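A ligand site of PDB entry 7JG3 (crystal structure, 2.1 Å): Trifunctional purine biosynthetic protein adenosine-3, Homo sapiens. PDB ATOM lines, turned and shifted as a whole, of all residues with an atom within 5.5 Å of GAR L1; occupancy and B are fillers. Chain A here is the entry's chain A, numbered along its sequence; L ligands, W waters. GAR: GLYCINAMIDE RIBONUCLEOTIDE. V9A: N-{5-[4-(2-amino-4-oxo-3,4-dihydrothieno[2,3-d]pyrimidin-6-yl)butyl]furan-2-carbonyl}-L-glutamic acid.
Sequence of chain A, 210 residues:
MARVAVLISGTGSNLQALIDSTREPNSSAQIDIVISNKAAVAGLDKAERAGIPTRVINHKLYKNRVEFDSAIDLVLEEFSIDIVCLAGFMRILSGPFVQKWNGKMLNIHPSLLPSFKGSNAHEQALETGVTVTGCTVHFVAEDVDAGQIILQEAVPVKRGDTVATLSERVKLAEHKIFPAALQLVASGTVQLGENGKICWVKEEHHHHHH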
ATOM      1  N   GLY A  10     -31.295  10.552 -16.672  1.00  0.00           N
ATOM      2  CA  GLY A  10     -32.186   9.582 -16.068  1.00  0.00           C
ATOM      3  C   GLY A  10     -33.004  10.086 -14.897  1.00  0.00           C
ATOM      4  O   GLY A  10     -33.782  11.023 -15.041  1.00  0.00           O
ATOM      5  N   THR A  11     -32.809   9.472 -13.728  1.00  0.00           N
ATOM      6  CA  THR A  11     -33.776   9.605 -12.632  1.00  0.00           C
ATOM      7  C   THR A  11     -33.869  11.040 -12.117  1.00  0.00           C
ATOM      8  O   THR A  11     -34.963  11.555 -11.881  1.00  0.00           O
ATOM      9  CB  THR A  11     -33.405   8.661 -11.502  1.00  0.00           C
ATOM     10  OG1 THR A  11     -33.293   7.324 -12.017  1.00  0.00           O
ATOM     11  CG2 THR A  11     -34.486   8.689 -10.428  1.00  0.00           C
ATOM     12  N   GLY A  12     -32.726  11.690 -11.905  1.00  0.00           N
ATOM     13  CA  GLY A  12     -32.723  13.073 -11.513  1.00  0.00           C
ATOM     14  C   GLY A  12     -32.808  13.333 -10.024  1.00  0.00           C
ATOM     15  O   GLY A  12     -33.296  14.405  -9.621  1.00  0.00           O
ATOM     16  N   SER A  13     -32.354  12.396  -9.195  1.00  0.00           N
ATOM     17  CA  SER A  13     -32.315  12.677  -7.755  1.00  0.00           C
ATOM     18  C   SER A  13     -31.353  13.822  -7.441  1.00  0.00           C
ATOM     19  O   SER A  13     -31.624  14.636  -6.551  1.00  0.00           O
ATOM     20  CB  SER A  13     -31.957  11.406  -6.982  1.00  0.00           C
ATOM     21  OG  SER A  13     -30.581  11.092  -7.081  1.00  0.00           O
ATOM     22  N   ASN A  14     -30.237  13.913  -8.165  1.00  0.00           N
ATOM     23  CA  ASN A  14     -29.346  15.049  -7.953  1.00  0.00           C
ATOM     24  C   ASN A  14     -30.019  16.342  -8.415  1.00  0.00           C
ATOM     25  O   ASN A  14     -29.968  17.355  -7.699  1.00  0.00           O
ATOM     26  CB  ASN A  14     -28.015  14.843  -8.679  1.00  0.00           C
ATOM     27  CG  ASN A  14     -27.033  14.028  -7.848  1.00  0.00           C
ATOM     28  OD1 ASN A  14     -26.413  14.543  -6.911  1.00  0.00           O
ATOM     29  ND2 ASN A  14     -26.889  12.764  -8.179  1.00  0.00           N
ATOM     30  N   LEU A  15     -30.673  16.298  -9.575  1.00  0.00           N
ATOM     31  CA  LEU A  15     -31.500  17.432 -10.003  1.00  0.00           C
ATOM     32  C   LEU A  15     -32.427  17.911  -8.894  1.00  0.00           C
ATOM     33  O   LEU A  15     -32.468  19.101  -8.562  1.00  0.00           O
ATOM     34  CB  LEU A  15     -32.326  17.045 -11.232  1.00  0.00           C
ATOM     35  CG  LEU A  15     -33.367  18.103 -11.597  1.00  0.00           C
ATOM     36  CD1 LEU A  15     -32.665  19.414 -11.892  1.00  0.00           C
ATOM     37  CD2 LEU A  15     -34.227  17.677 -12.802  1.00  0.00           C
ATOM     38  N   ALA A  87     -25.796  16.402 -14.001  1.00  0.00           N
ATOM     39  CA  ALA A  87     -26.419  15.696 -12.884  1.00  0.00           C
ATOM     40  C   ALA A  87     -26.959  14.377 -13.429  1.00  0.00           C
ATOM     41  O   ALA A  87     -28.131  14.269 -13.781  1.00  0.00           O
ATOM     42  CB  ALA A  87     -27.546  16.536 -12.232  1.00  0.00           C
ATOM     43  N   GLY A  88     -26.082  13.377 -13.507  1.00  0.00           N
ATOM     44  CA  GLY A  88     -26.451  12.124 -14.135  1.00  0.00           C
ATOM     45  C   GLY A  88     -26.441  12.169 -15.639  1.00  0.00           C
ATOM     46  O   GLY A  88     -27.032  11.287 -16.273  1.00  0.00           O
ATOM     47  N   PHE A  89     -25.811  13.178 -16.225  1.00  0.00           N
ATOM     48  CA  PHE A  89     -25.636  13.262 -17.668  1.00  0.00           C
ATOM     49  C   PHE A  89     -24.507  12.341 -18.080  1.00  0.00           C
ATOM     50  O   PHE A  89     -23.389  12.440 -17.567  1.00  0.00           O
ATOM     51  CB  PHE A  89     -25.337  14.707 -18.060  1.00  0.00           C
ATOM     52  CG  PHE A  89     -25.370  14.968 -19.528  1.00  0.00           C
ATOM     53  CD1 PHE A  89     -26.576  14.994 -20.208  1.00  0.00           C
ATOM     54  CD2 PHE A  89     -24.197  15.180 -20.234  1.00  0.00           C
ATOM     55  CE1 PHE A  89     -26.610  15.234 -21.574  1.00  0.00           C
ATOM     56  CE2 PHE A  89     -24.222  15.417 -21.599  1.00  0.00           C
ATOM     57  CZ  PHE A  89     -25.425  15.454 -22.270  1.00  0.00           C
ATOM     58  N   MET A  90     -24.786  11.429 -19.005  1.00  0.00           N
ATOM     59  CA  MET A  90     -23.868  10.325 -19.261  1.00  0.00           C
ATOM     60  C   MET A  90     -23.146  10.442 -20.603  1.00  0.00           C
ATOM     61  O   MET A  90     -22.487   9.485 -21.013  1.00  0.00           O
ATOM     62  CB  MET A  90     -24.608   8.984 -19.175  1.00  0.00           C
ATOM     63  CG  MET A  90     -25.067   8.603 -17.778  1.00  0.00           C
ATOM     64  SD  MET A  90     -23.823   8.902 -16.468  1.00  0.00           S
ATOM     65  CE  MET A  90     -22.611   7.632 -16.859  1.00  0.00           C
ATOM     66  N   ASN A 107     -19.684  18.733 -12.598  1.00  0.00           N
ATOM     67  CA  ASN A 107     -20.150  17.361 -12.723  1.00  0.00           C
ATOM     68  C   ASN A 107     -20.056  16.693 -11.349  1.00  0.00           C
ATOM     69  O   ASN A 107     -19.140  16.975 -10.580  1.00  0.00           O
ATOM     70  CB  ASN A 107     -19.315  16.593 -13.743  1.00  0.00           C
ATOM     71  CG  ASN A 107     -19.675  15.132 -13.804  1.00  0.00           C
ATOM     72  OD1 ASN A 107     -20.821  14.769 -14.098  1.00  0.00           O
ATOM     73  ND2 ASN A 107     -18.704  14.277 -13.513  1.00  0.00           N
ATOM     74  N   ILE A 108     -21.034  15.825 -11.049  1.00  0.00           N
ATOM     75  CA  ILE A 108     -21.013  14.983  -9.850  1.00  0.00           C
ATOM     76  C   ILE A 108     -20.566  13.596 -10.280  1.00  0.00           C
ATOM     77  O   ILE A 108     -21.072  13.032 -11.258  1.00  0.00           O
ATOM     78  CB  ILE A 108     -22.395  14.939  -9.159  1.00  0.00           C
ATOM     79  CG1 ILE A 108     -22.398  14.026  -7.912  1.00  0.00           C
ATOM     80  CG2 ILE A 108     -23.494  14.434 -10.100  1.00  0.00           C
ATOM     81  CD1 ILE A 108     -21.720  14.584  -6.686  1.00  0.00           C
ATOM     82  N   HIS A 109     -19.585  13.031  -9.577  1.00  0.00           N
ATOM     83  CA  HIS A 109     -19.088  11.720  -9.933  1.00  0.00           C
ATOM     84  C   HIS A 109     -19.074  10.867  -8.662  1.00  0.00           C
ATOM     85  O   HIS A 109     -18.572  11.324  -7.612  1.00  0.00           O
ATOM     86  CB  HIS A 109     -17.701  11.791 -10.557  1.00  0.00           C
ATOM     87  CG  HIS A 109     -17.112  10.445 -10.867  1.00  0.00           C
ATOM     88  ND1 HIS A 109     -17.343   9.787 -12.049  1.00  0.00           N
ATOM     89  CD2 HIS A 109     -16.299   9.641 -10.133  1.00  0.00           C
ATOM     90  CE1 HIS A 109     -16.704   8.638 -12.037  1.00  0.00           C
ATOM     91  NE2 HIS A 109     -16.055   8.524 -10.889  1.00  0.00           N
ATOM     92  N   PRO A 110     -19.619   9.664  -8.707  1.00  0.00           N
ATOM     93  CA  PRO A 110     -19.833   8.842  -7.506  1.00  0.00           C
ATOM     94  C   PRO A 110     -18.599   8.058  -7.064  1.00  0.00           C
ATOM     95  O   PRO A 110     -18.658   6.863  -6.804  1.00  0.00           O
ATOM     96  CB  PRO A 110     -20.965   7.903  -7.947  1.00  0.00           C
ATOM     97  CG  PRO A 110     -20.699   7.666  -9.384  1.00  0.00           C
ATOM     98  CD  PRO A 110     -20.124   8.991  -9.925  1.00  0.00           C
ATOM     99  N   GLY A 118     -14.706   7.109 -14.793  1.00  0.00           N
ATOM    100  CA  GLY A 118     -15.503   6.384 -15.752  1.00  0.00           C
ATOM    101  C   GLY A 118     -16.912   6.108 -15.248  1.00  0.00           C
ATOM    102  O   GLY A 118     -17.351   6.599 -14.207  1.00  0.00           O
ATOM    103  N   SER A 119     -17.616   5.281 -16.002  1.00  0.00           N
ATOM    104  CA  SER A 119     -19.059   5.194 -15.911  1.00  0.00           C
ATOM    105  C   SER A 119     -19.569   4.182 -14.889  1.00  0.00           C
ATOM    106  O   SER A 119     -20.769   4.178 -14.599  1.00  0.00           O
ATOM    107  CB  SER A 119     -19.647   4.836 -17.287  1.00  0.00           C
ATOM    108  OG  SER A 119     -19.141   3.579 -17.699  1.00  0.00           O
ATOM    109  N   HIS A 122     -19.065   2.594  -8.915  1.00  0.00           N
ATOM    110  CA  HIS A 122     -19.436   1.714  -7.823  1.00  0.00           C
ATOM    111  C   HIS A 122     -18.923   0.304  -8.067  1.00  0.00           C
ATOM    112  O   HIS A 122     -18.350  -0.325  -7.157  1.00  0.00           O
ATOM    113  CB  HIS A 122     -20.946   1.699  -7.641  1.00  0.00           C
ATOM    114  CG  HIS A 122     -21.486   3.022  -7.207  1.00  0.00           C
ATOM    115  ND1 HIS A 122     -20.919   3.730  -6.172  1.00  0.00           N
ATOM    116  CD2 HIS A 122     -22.539   3.751  -7.637  1.00  0.00           C
ATOM    117  CE1 HIS A 122     -21.596   4.857  -6.002  1.00  0.00           C
ATOM    118  NE2 HIS A 122     -22.581   4.880  -6.877  1.00  0.00           N
ATOM    119  N   ASP A 145     -13.327  13.274 -15.943  1.00  0.00           N
ATOM    120  CA  ASP A 145     -13.214  13.071 -14.488  1.00  0.00           C
ATOM    121  C   ASP A 145     -11.857  13.519 -13.957  1.00  0.00           C
ATOM    122  O   ASP A 145     -11.322  12.948 -13.004  1.00  0.00           O
ATOM    123  CB  ASP A 145     -13.486  11.606 -14.114  1.00  0.00           C
ATOM    124  CG  ASP A 145     -14.895  11.163 -14.437  1.00  0.00           C
ATOM    125  OD1 ASP A 145     -15.799  12.037 -14.537  1.00  0.00           O
ATOM    126  OD2 ASP A 145     -15.118   9.934 -14.590  1.00  0.00           O
ATOM    127  N   LYS A 171     -25.482   8.367  -2.849  1.00  0.00           N
ATOM    128  CA  LYS A 171     -26.331   9.446  -3.363  1.00  0.00           C
ATOM    129  C   LYS A 171     -26.744  10.418  -2.263  1.00  0.00           C
ATOM    130  O   LYS A 171     -26.938  11.606  -2.529  1.00  0.00           O
ATOM    131  CB  LYS A 171     -27.553   8.885  -4.080  1.00  0.00           C
ATOM    132  CG  LYS A 171     -27.337   8.678  -5.581  1.00  0.00           C
ATOM    133  CD  LYS A 171     -28.475   7.832  -6.164  1.00  0.00           C
ATOM    134  CE  LYS A 171     -28.291   7.551  -7.668  1.00  0.00           C
ATOM    135  NZ  LYS A 171     -29.612   7.459  -8.408  1.00  0.00           N
ATOM    136  N   GLU A 174     -24.096  12.752  -2.355  1.00  0.00           N
ATOM    137  CA  GLU A 174     -24.170  13.555  -3.572  1.00  0.00           C
ATOM    138  C   GLU A 174     -25.142  14.708  -3.412  1.00  0.00           C
ATOM    139  O   GLU A 174     -24.831  15.845  -3.800  1.00  0.00           O
ATOM    140  CB  GLU A 174     -24.571  12.677  -4.744  1.00  0.00           C
ATOM    141  CG  GLU A 174     -23.477  11.697  -5.211  1.00  0.00           C
ATOM    142  CD  GLU A 174     -24.020  10.774  -6.323  1.00  0.00           C
ATOM    143  OE1 GLU A 174     -23.518   9.659  -6.489  1.00  0.00           O
ATOM    144  OE2 GLU A 174     -24.965  11.180  -7.027  1.00  0.00           O
ATOM    145  N   HIS A 175     -26.303  14.440  -2.811  1.00  0.00           N
ATOM    146  CA  HIS A 175     -27.322  15.470  -2.660  1.00  0.00           C
ATOM    147  C   HIS A 175     -26.941  16.526  -1.658  1.00  0.00           C
ATOM    148  O   HIS A 175     -27.692  17.505  -1.514  1.00  0.00           O
ATOM    149  CB  HIS A 175     -28.636  14.831  -2.244  1.00  0.00           C
ATOM    150  CG  HIS A 175     -29.104  13.777  -3.178  1.00  0.00           C
ATOM    151  ND1 HIS A 175     -30.030  12.813  -2.826  1.00  0.00           N
ATOM    152  CD2 HIS A 175     -28.758  13.520  -4.469  1.00  0.00           C
ATOM    153  CE1 HIS A 175     -30.238  12.017  -3.852  1.00  0.00           C
ATOM    154  NE2 HIS A 175     -29.482  12.420  -4.861  1.00  0.00           N
HETATM  155  C1  GAR L   1     -25.351   9.688  -9.763  1.00  0.00           C
HETATM  156  O6  GAR L   1     -25.082   8.684  -8.800  1.00  0.00           O
HETATM  157  C2  GAR L   1     -24.000  10.174 -10.332  1.00  0.00           C
HETATM  158  O8  GAR L   1     -22.975  10.126  -9.373  1.00  0.00           O
HETATM  159  C3  GAR L   1     -23.797   9.243 -11.553  1.00  0.00           C
HETATM  160  O4  GAR L   1     -25.138   8.934 -12.009  1.00  0.00           O
HETATM  161  C5  GAR L   1     -26.117   9.087 -10.956  1.00  0.00           C
HETATM  162  C10 GAR L   1     -27.303   9.930 -11.392  1.00  0.00           C
HETATM  163  O12 GAR L   1     -28.346   9.853 -10.416  1.00  0.00           O
HETATM  164  N19 GAR L   1     -23.011   9.765 -12.645  1.00  0.00           N
HETATM  165  C21 GAR L   1     -21.912   9.094 -13.055  1.00  0.00           C
HETATM  166  O22 GAR L   1     -21.619   7.935 -12.729  1.00  0.00           O
HETATM  167  C23 GAR L   1     -21.033   9.887 -13.993  1.00  0.00           C
HETATM  168  N24 GAR L   1     -19.921   9.127 -14.523  1.00  0.00           N
HETATM  169  P15 GAR L   1     -29.623  10.838 -10.549  1.00  0.00           P
HETATM  170  O16 GAR L   1     -29.046  12.185 -10.137  1.00  0.00           O
HETATM  171  O17 GAR L   1     -30.657  10.262  -9.599  1.00  0.00           O
HETATM  172  O18 GAR L   1     -30.008  10.724 -12.007  1.00  0.00           O
HETATM  173  O25 V9A L   2     -24.733   5.932 -20.445  1.00  0.00           O
HETATM  174  C26 V9A L   2     -20.562   8.403 -24.153  1.00  0.00           C
HETATM  175  C30 V9A L   2     -20.516  14.100 -17.106  1.00  0.00           C
HETATM  176  C32 V9A L   2     -19.461  11.860 -17.275  1.00  0.00           C
HETATM  177  C31 V9A L   2     -20.307  12.774 -16.392  1.00  0.00           C
HETATM  178  C33 V9A L   2     -20.150  10.515 -17.378  1.00  0.00           C
HETATM  179  C20 V9A L   2     -20.763   7.355 -23.068  1.00  0.00           C
HETATM  180  C16 V9A L   2     -19.332   9.523 -18.183  1.00  0.00           C
HETATM  181  C17 V9A L   2     -19.194   7.531 -21.162  1.00  0.00           C
HETATM  182  C22 V9A L   2     -22.667   6.453 -21.623  1.00  0.00           C
HETATM  183  C21 V9A L   2     -22.255   7.032 -22.973  1.00  0.00           C
HETATM  184  C13 V9A L   2     -18.905   8.207 -19.829  1.00  0.00           C
HETATM  185  C8  V9A L   2     -17.054  15.015 -18.490  1.00  0.00           C
HETATM  186  C9  V9A L   2     -17.606  15.043 -19.776  1.00  0.00           C
HETATM  187  C4  V9A L   2     -15.667  15.306 -18.383  1.00  0.00           C
HETATM  188  C14 V9A L   2     -17.789   8.089 -18.980  1.00  0.00           C
HETATM  189  C15 V9A L   2     -18.085   8.963 -17.876  1.00  0.00           C
HETATM  190  C2  V9A L   2     -15.580  15.598 -20.636  1.00  0.00           C
HETATM  191  C23 V9A L   2     -24.161   6.117 -21.566  1.00  0.00           C
HETATM  192  C6  V9A L   2     -19.317  14.450 -17.916  1.00  0.00           C
HETATM  193  C7  V9A L   2     -18.016  14.669 -17.432  1.00  0.00           C
HETATM  194  N1  V9A L   2     -16.877  15.342 -20.855  1.00  0.00           N
HETATM  195  N11 V9A L   2     -14.844  15.885 -21.714  1.00  0.00           N
HETATM  196  N19 V9A L   2     -20.325   7.886 -21.795  1.00  0.00           N
HETATM  197  N3  V9A L   2     -14.931  15.593 -19.460  1.00  0.00           N
HETATM  198  O10 V9A L   2     -15.137  15.280 -17.248  1.00  0.00           O
HETATM  199  O12 V9A L   2     -19.752   9.043 -19.310  1.00  0.00           O
HETATM  200  O18 V9A L   2     -18.426   6.682 -21.632  1.00  0.00           O
HETATM  201  O24 V9A L   2     -24.823   6.032 -22.632  1.00  0.00           O
HETATM  202  O27 V9A L   2     -21.007   8.155 -25.456  1.00  0.00           O
HETATM  203  O28 V9A L   2     -19.941   9.628 -23.867  1.00  0.00           O
HETATM  204  S5  V9A L   2     -19.276  14.663 -19.639  1.00  0.00           S
HETATM  205  O   HOH W   1     -29.803  11.930 -14.638  1.00  0.00           O
HETATM  206  O   HOH W   2     -30.016   8.437 -13.156  1.00  0.00           O
HETATM  207  O   HOH W   3     -30.036  14.314 -11.595  1.00  0.00           O
HETATM  208  O   HOH W   4     -25.928   6.756 -13.705  1.00  0.00           O
HETATM  209  O   HOH W   5     -24.720   6.049  -9.146  1.00  0.00           O
HETATM  210  O   HOH W   6     -24.294   6.902  -6.068  1.00  0.00           O
HETATM  211  O   HOH W   7     -19.356   6.089 -12.425  1.00  0.00           O
HETATM  212  O   HOH W   8     -23.324  12.777 -12.993  1.00  0.00           O
HETATM  213  O   HOH W   9     -18.094  11.318 -14.028  1.00  0.00           O
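N of Pro 110 lies close to O8 of GAR L1, 3.5 Å away. Residues that only touch GAR L1: Thr 11, Gly 88, Gly 118, His 109, Met 90 and Ile 108. Hydrophobic or aromatic side chains that line GAR L1: Met 90 and Pro 110. 12 residues have an atom within 4 Å of GAR L1: Thr 11, Gly 12, Ser 13, Asn 14, Gly 88, Met 90, Ile 108, His 109, Pro 110, Gly 118, Lys 171 and Glu 174. The nearest printed residue that does not touch GAR L1 is Gly 10 (4.2 Å).
Water W2 bridges an oxygen (O18) of GAR L1 (2.6 Å) and the backbone NH (N) of Thr 11 (3.0 Å). Water W5 bridges O6 of GAR L1 (2.7 Å) and NE2 of His 122 (3.3 Å). Water W3 lies within hydrogen-bond range of an oxygen (O16) of GAR L1 (2.8 Å), the backbone carbonyl oxygen of Ala 87 (2.9 Å), the backbone NH of Leu 15 (2.9 Å) and the backbone NH of Asn 14 (3.5 Å). Water W9 lies within hydrogen-bond range of the side-chain carboxylate of Asp 145, a ring nitrogen (ND1) of His 109, a nitrogen (N24) of GAR L1 and the side-chain amide nitrogen of Asn 107. Water W1 lies within hydrogen-bond range of N of Gly 10 (2.9 Å), O18 of GAR L1 (2.9 Å), O of Ala 87 (3.0 Å) and O of Gly 88 (3.3 Å). Water W6 lies within hydrogen-bond range of a ring nitrogen (NE2) of His 122 (2.8 Å), the side-chain carboxylate (OE1) of Glu 174 (2.9 Å) and an oxygen (O6) of GAR L1 (3.4 Å).
The backbone NH of Gly 118 is in hydrogen-bond range of the side-chain carboxylate of Asp 145, at 2.9 Å. The side-chain amide nitrogen (ND2) of Asn 14 lies within hydrogen-bond range of the side-chain carboxylate (OE2) of Glu 174 (2.7 Å). A ring nitrogen (NE2) of His 175 sits at hydrogen-bond distance from the side-chain hydroxyl (OG) of Ser 13 (2.8 Å). The backbone carbonyl oxygen (O) of Lys 171 lies close to a ring nitrogen (ND1) of His 175 (3.3 Å). OD2 of Asp 145 sits close to ND1 of His 109, at 3.4 Å.
O of Met 90 sits at hydrogen-bond distance from N19 of V9A L2 (2.8 Å). NZ of Lys 171 lies within salt-bridge range of O17 of GAR L1, 3.2 Å away. The backbone NH (N) of Gly 12 sits at hydrogen-bond distance from an oxygen (O18) of GAR L1, at 2.9 Å. An oxygen (O10) of V9A L2 is in hydrogen-bond range of the backbone NH (N) of Asp 145 (3.0 Å). The side-chain carboxylate (OE1) of Glu 174 sits at hydrogen-bond distance from an oxygen (O6) of GAR L1 (3.0 Å). An oxygen (O17) of GAR L1 is in hydrogen-bond range of the side-chain hydroxyl (OG) of Ser 13. O17 of GAR L1 lies within hydrogen-bond range of N of Ser 13 (2.8 Å). The side-chain amide nitrogen of Asn 14 sits at hydrogen-bond distance from an oxygen (O16) of GAR L1 (3.0 Å). The backbone NH (N) of Asn 14 is in hydrogen-bond range of an oxygen (O16) of GAR L1 (2.9 Å).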
